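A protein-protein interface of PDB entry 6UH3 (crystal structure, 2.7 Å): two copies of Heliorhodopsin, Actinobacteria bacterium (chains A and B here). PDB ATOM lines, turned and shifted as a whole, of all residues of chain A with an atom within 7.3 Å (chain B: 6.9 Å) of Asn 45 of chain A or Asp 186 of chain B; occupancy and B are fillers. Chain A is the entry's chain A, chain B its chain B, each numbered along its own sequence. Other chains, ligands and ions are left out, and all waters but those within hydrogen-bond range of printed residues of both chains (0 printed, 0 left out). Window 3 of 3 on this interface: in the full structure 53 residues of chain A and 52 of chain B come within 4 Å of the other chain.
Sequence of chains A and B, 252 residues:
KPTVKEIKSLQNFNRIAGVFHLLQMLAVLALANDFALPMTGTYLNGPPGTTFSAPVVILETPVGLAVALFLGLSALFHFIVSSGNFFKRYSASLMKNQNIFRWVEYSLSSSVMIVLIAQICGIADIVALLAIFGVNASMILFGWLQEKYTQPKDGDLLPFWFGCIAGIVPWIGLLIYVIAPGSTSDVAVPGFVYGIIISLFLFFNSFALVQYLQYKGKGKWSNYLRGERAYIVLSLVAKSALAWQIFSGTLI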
ATOM      1  N   THR A  42       1.867  34.922 -13.738  1.00  0.00           N
ATOM      2  CA  THR A  42       2.564  34.111 -14.736  1.00  0.00           C
ATOM      3  C   THR A  42       3.863  33.605 -14.109  1.00  0.00           C
ATOM      4  O   THR A  42       4.920  34.239 -14.222  1.00  0.00           O
ATOM      5  CB  THR A  42       2.826  34.893 -16.028  1.00  0.00           C
ATOM      6  OG1 THR A  42       1.586  35.410 -16.535  1.00  0.00           O
ATOM      7  CG2 THR A  42       3.431  33.975 -17.070  1.00  0.00           C
ATOM      8  N   TYR A  43       3.751  32.465 -13.432  1.00  0.00           N
ATOM      9  CA  TYR A  43       4.800  31.861 -12.628  1.00  0.00           C
ATOM     10  C   TYR A  43       5.831  31.181 -13.529  1.00  0.00           C
ATOM     11  O   TYR A  43       5.578  30.922 -14.706  1.00  0.00           O
ATOM     12  CB  TYR A  43       4.188  30.828 -11.686  1.00  0.00           C
ATOM     13  CG  TYR A  43       3.025  31.342 -10.851  1.00  0.00           C
ATOM     14  CD1 TYR A  43       3.195  32.361  -9.927  1.00  0.00           C
ATOM     15  CD2 TYR A  43       1.757  30.785 -11.001  1.00  0.00           C
ATOM     16  CE1 TYR A  43       2.129  32.826  -9.190  1.00  0.00           C
ATOM     17  CE2 TYR A  43       0.687  31.232 -10.248  1.00  0.00           C
ATOM     18  CZ  TYR A  43       0.879  32.257  -9.346  1.00  0.00           C
ATOM     19  OH  TYR A  43      -0.172  32.709  -8.578  1.00  0.00           O
ATOM     20  N   LEU A  44       6.994  30.855 -12.956  1.00  0.00           N
ATOM     21  CA  LEU A  44       8.029  30.147 -13.706  1.00  0.00           C
ATOM     22  C   LEU A  44       7.810  28.630 -13.745  1.00  0.00           C
ATOM     23  O   LEU A  44       7.344  28.023 -12.777  1.00  0.00           O
ATOM     24  CB  LEU A  44       9.406  30.439 -13.100  1.00  0.00           C
ATOM     25  CG  LEU A  44       9.965  31.859 -13.175  1.00  0.00           C
ATOM     26  CD1 LEU A  44      11.225  31.958 -12.331  1.00  0.00           C
ATOM     27  CD2 LEU A  44      10.261  32.258 -14.610  1.00  0.00           C
ATOM     28  N   ASN A  45       8.198  28.017 -14.872  1.00  0.00           N
ATOM     29  CA  ASN A  45       8.274  26.567 -15.032  1.00  0.00           C
ATOM     30  C   ASN A  45       9.684  26.055 -14.818  1.00  0.00           C
ATOM     31  O   ASN A  45      10.005  24.936 -15.241  1.00  0.00           O
ATOM     32  CB  ASN A  45       7.838  26.115 -16.426  1.00  0.00           C
ATOM     33  CG  ASN A  45       6.358  25.982 -16.578  1.00  0.00           C
ATOM     34  OD1 ASN A  45       5.775  26.519 -17.519  1.00  0.00           O
ATOM     35  ND2 ASN A  45       5.732  25.247 -15.668  1.00  0.00           N
ATOM     36  N   GLY A  46      10.538  26.868 -14.220  1.00  0.00           N
ATOM     37  CA  GLY A  46      11.923  26.525 -14.074  1.00  0.00           C
ATOM     38  C   GLY A  46      12.787  27.754 -13.865  1.00  0.00           C
ATOM     39  O   GLY A  46      12.484  28.647 -13.071  1.00  0.00           O
ATOM     40  N   PRO A  47      13.914  27.765 -14.579  1.00  0.00           N
ATOM     41  CA  PRO A  47      14.876  28.858 -14.463  1.00  0.00           C
ATOM     42  C   PRO A  47      14.323  30.199 -14.915  1.00  0.00           C
ATOM     43  O   PRO A  47      13.487  30.280 -15.836  1.00  0.00           O
ATOM     44  CB  PRO A  47      16.034  28.402 -15.361  1.00  0.00           C
ATOM     45  CG  PRO A  47      15.945  26.917 -15.337  1.00  0.00           C
ATOM     46  CD  PRO A  47      14.488  26.575 -15.237  1.00  0.00           C
ATOM     47  N   THR A  50      14.392  30.944 -18.663  1.00  0.00           N
ATOM     48  CA  THR A  50      14.100  29.787 -19.502  1.00  0.00           C
ATOM     49  C   THR A  50      12.615  29.652 -19.835  1.00  0.00           C
ATOM     50  O   THR A  50      12.251  29.634 -21.014  1.00  0.00           O
ATOM     51  CB  THR A  50      14.608  28.495 -18.849  1.00  0.00           C
ATOM     52  OG1 THR A  50      16.031  28.549 -18.720  1.00  0.00           O
ATOM     53  CG2 THR A  50      14.240  27.293 -19.713  1.00  0.00           C
ATOM     54  N   THR A  51      11.739  29.577 -18.830  1.00  0.00           N
ATOM     55  CA  THR A  51      10.351  29.279 -19.165  1.00  0.00           C
ATOM     56  C   THR A  51       9.346  29.731 -18.110  1.00  0.00           C
ATOM     57  O   THR A  51       9.648  29.785 -16.915  1.00  0.00           O
ATOM     58  CB  THR A  51      10.198  27.772 -19.407  1.00  0.00           C
ATOM     59  OG1 THR A  51       8.830  27.468 -19.699  1.00  0.00           O
ATOM     60  CG2 THR A  51      10.696  26.982 -18.201  1.00  0.00           C
ATOM     61  N   PHE A  52       8.130  30.032 -18.587  1.00  0.00           N
ATOM     62  CA  PHE A  52       7.012  30.508 -17.779  1.00  0.00           C
ATOM     63  C   PHE A  52       5.780  29.615 -17.903  1.00  0.00           C
ATOM     64  O   PHE A  52       5.431  29.172 -19.002  1.00  0.00           O
ATOM     65  CB  PHE A  52       6.580  31.927 -18.183  1.00  0.00           C
ATOM     66  CG  PHE A  52       7.570  33.006 -17.869  1.00  0.00           C
ATOM     67  CD1 PHE A  52       8.702  33.188 -18.645  1.00  0.00           C
ATOM     68  CD2 PHE A  52       7.331  33.885 -16.831  1.00  0.00           C
ATOM     69  CE1 PHE A  52       9.594  34.208 -18.360  1.00  0.00           C
ATOM     70  CE2 PHE A  52       8.214  34.906 -16.544  1.00  0.00           C
ATOM     71  CZ  PHE A  52       9.349  35.068 -17.307  1.00  0.00           C
ATOM     72  N   SER A  53       5.100  29.405 -16.775  1.00  0.00           N
ATOM     73  CA  SER A  53       3.815  28.716 -16.736  1.00  0.00           C
ATOM     74  C   SER A  53       2.718  29.648 -17.228  1.00  0.00           C
ATOM     75  O   SER A  53       2.727  30.843 -16.932  1.00  0.00           O
ATOM     76  CB  SER A  53       3.488  28.236 -15.323  1.00  0.00           C
ATOM     77  OG  SER A  53       2.239  27.563 -15.293  1.00  0.00           O
ATOM     78  N   ALA A  54       1.773  29.095 -17.979  1.00  0.00           N
ATOM     79  CA  ALA A  54       0.703  29.898 -18.559  1.00  0.00           C
ATOM     80  C   ALA A  54      -0.084  30.646 -17.481  1.00  0.00           C
ATOM     81  O   ALA A  54      -0.348  30.094 -16.403  1.00  0.00           O
ATOM     82  CB  ALA A  54      -0.240  29.012 -19.377  1.00  0.00           C
ATOM     83  N   VAL A  56      -2.362  32.121 -14.753  1.00  0.00           N
ATOM     84  CA  VAL A  56      -3.463  31.590 -13.960  1.00  0.00           C
ATOM     85  C   VAL A  56      -4.170  32.742 -13.261  1.00  0.00           C
ATOM     86  O   VAL A  56      -3.535  33.572 -12.597  1.00  0.00           O
ATOM     87  CB  VAL A  56      -2.970  30.542 -12.951  1.00  0.00           C
ATOM     88  CG1 VAL A  56      -4.115  30.098 -12.071  1.00  0.00           C
ATOM     89  CG2 VAL A  56      -2.421  29.357 -13.700  1.00  0.00           C
ATOM     90  N   GLY B 182      -2.081  30.208  -7.551  1.00  0.00           N
ATOM     91  CA  GLY B 182      -2.762  29.525  -8.634  1.00  0.00           C
ATOM     92  C   GLY B 182      -1.950  28.409  -9.262  1.00  0.00           C
ATOM     93  O   GLY B 182      -2.267  27.967 -10.369  1.00  0.00           O
ATOM     94  N   SER B 183      -0.907  27.947  -8.569  1.00  0.00           N
ATOM     95  CA  SER B 183      -0.036  26.899  -9.092  1.00  0.00           C
ATOM     96  C   SER B 183      -0.818  25.668  -9.519  1.00  0.00           C
ATOM     97  O   SER B 183      -1.723  25.204  -8.820  1.00  0.00           O
ATOM     98  CB  SER B 183       0.997  26.485  -8.045  1.00  0.00           C
ATOM     99  OG  SER B 183       1.699  25.333  -8.476  1.00  0.00           O
ATOM    100  N   THR B 184      -0.442  25.135 -10.683  1.00  0.00           N
ATOM    101  CA  THR B 184      -1.038  23.925 -11.232  1.00  0.00           C
ATOM    102  C   THR B 184      -0.054  22.752 -11.262  1.00  0.00           C
ATOM    103  O   THR B 184      -0.181  21.855 -12.098  1.00  0.00           O
ATOM    104  CB  THR B 184      -1.614  24.220 -12.619  1.00  0.00           C
ATOM    105  OG1 THR B 184      -0.628  24.867 -13.438  1.00  0.00           O
ATOM    106  CG2 THR B 184      -2.850  25.118 -12.510  1.00  0.00           C
ATOM    107  N   SER B 185       0.916  22.755 -10.332  1.00  0.00           N
ATOM    108  CA  SER B 185       1.909  21.712 -10.043  1.00  0.00           C
ATOM    109  C   SER B 185       3.125  21.674 -10.968  1.00  0.00           C
ATOM    110  O   SER B 185       4.155  21.085 -10.615  1.00  0.00           O
ATOM    111  CB  SER B 185       1.256  20.325 -10.063  1.00  0.00           C
ATOM    112  OG  SER B 185       1.227  19.806 -11.383  1.00  0.00           O
ATOM    113  N   ASP B 186       3.038  22.308 -12.134  1.00  0.00           N
ATOM    114  CA  ASP B 186       4.176  22.422 -13.039  1.00  0.00           C
ATOM    115  C   ASP B 186       5.118  23.551 -12.642  1.00  0.00           C
ATOM    116  O   ASP B 186       6.242  23.625 -13.157  1.00  0.00           O
ATOM    117  CB  ASP B 186       3.668  22.634 -14.466  1.00  0.00           C
ATOM    118  CG  ASP B 186       2.747  23.831 -14.578  1.00  0.00           C
ATOM    119  OD1 ASP B 186       1.750  23.876 -13.831  1.00  0.00           O
ATOM    120  OD2 ASP B 186       2.994  24.719 -15.418  1.00  0.00           O
ATOM    121  N   VAL B 187       4.686  24.401 -11.727  1.00  0.00           N
ATOM    122  CA  VAL B 187       5.430  25.571 -11.276  1.00  0.00           C
ATOM    123  C   VAL B 187       6.562  25.181 -10.336  1.00  0.00           C
ATOM    124  O   VAL B 187       6.394  24.340  -9.445  1.00  0.00           O
ATOM    125  CB  VAL B 187       4.468  26.564 -10.610  1.00  0.00           C
ATOM    126  CG1 VAL B 187       5.237  27.703  -9.984  1.00  0.00           C
ATOM    127  CG2 VAL B 187       3.506  27.094 -11.649  1.00  0.00           C
ATOM    128  N   ALA B 188       7.731  25.786 -10.541  1.00  0.00           N
ATOM    129  CA  ALA B 188       8.877  25.520  -9.687  1.00  0.00           C
ATOM    130  C   ALA B 188       9.774  26.749  -9.593  1.00  0.00           C
ATOM    131  O   ALA B 188      10.032  27.420 -10.594  1.00  0.00           O
ATOM    132  CB  ALA B 188       9.669  24.327 -10.220  1.00  0.00           C
ATOM    133  N   VAL B 189      10.258  27.026  -8.393  1.00  0.00           N
ATOM    134  CA  VAL B 189      11.197  28.119  -8.146  1.00  0.00           C
ATOM    135  C   VAL B 189      12.538  27.528  -7.721  1.00  0.00           C
ATOM    136  O   VAL B 189      12.567  26.597  -6.906  1.00  0.00           O
ATOM    137  CB  VAL B 189      10.673  29.103  -7.082  1.00  0.00           C
ATOM    138  CG1 VAL B 189      11.701  30.197  -6.826  1.00  0.00           C
ATOM    139  CG2 VAL B 189       9.369  29.728  -7.552  1.00  0.00           C
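The side-chain hydroxyl (OH) of Tyr 43 of chain A is in hydrogen-bond range of the backbone NH (N) of Gly 182 of chain B (3.3 Å).
N of Ala 188 of chain B sits at hydrogen-bond distance from O of Leu 44 of chain A (3.2 Å).
The side-chain carboxylate of Asp 186 of chain B sits at hydrogen-bond distance from the side-chain amide nitrogen of Asn 45 of chain A, 2.8 Å away.
OD2 of Asp 186 of chain B is in hydrogen-bond range of OG of Ser 53 of chain A (2.9 Å).
The backbone carbonyl oxygen (O) of Tyr 43 of chain A is in hydrogen-bond range of the backbone NH (N) of Ser 53 of chain A (2.6 Å).
The backbone NH (N) of Asn 45 of chain A is in hydrogen-bond range of the backbone carbonyl oxygen (O) of Thr 51 of chain A (3.1 Å).
The backbone carbonyl oxygen (O) of Phe 52 of chain A sits close to the side-chain amide oxygen (OD1) of Asn 45 of chain A, 3.1 Å away.
N of Ser 53 of chain A sits close to OD1 of Asn 45 of chain A.
The side-chain carboxylate of Asp 186 of chain B sits at hydrogen-bond distance from the side-chain hydroxyl of Thr 184 of chain B, at 2.6 Å.
Among the printed residues, merely in contact across the chains: Val 56 of chain A with Gly 182 of chain B, Leu 44 of chain A with Val 187 of chain B, Gly 46 of chain A with Ala 188 of chain B, Tyr 43 of chain A with Val 187 of chain B and Ser 53 of chain A with Val 187 of chain B.
Of chain B, only Asp 186 comes within 4 Å of Asn 45 of chain A.
Printed residues of chain B within 4 Å of Gly 46 of chain A: Ala 188 (3.7 Å).
Printed residues of chain B within 4 Å of Ser 53 of chain A: Asp 186 and Val 187.
Of the printed residues of chain A, Gly 182 of chain B touches Tyr 43 and Val 56.
Of chain A, only Asn 45 (2.8 Å) and Ser 53 (2.9 Å) come within 4 Å of Asp 186 of chain B.
The nearest residue of chain B that does not touch Asn 45 of chain A is Val 187 of chain B (4.2 Å).
The nearest printed residue of chain B that does not touch Ser 53 of chain A is Thr 184 of chain B (4.4 Å).
Hydrophobic or aromatic side chains of chain B within 4 Å of the printed part of chain A: Val 187.
Of the 12 printed residues of chain A, 6 touch a printed residue of chain B.
Hydrophobic or aromatic side chains of chain A that line the printed part of chain B: Tyr 43, Leu 44 and Val 56.
Among the printed residues, 9 pairs touch across the chains.
No position is printed for both chains.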
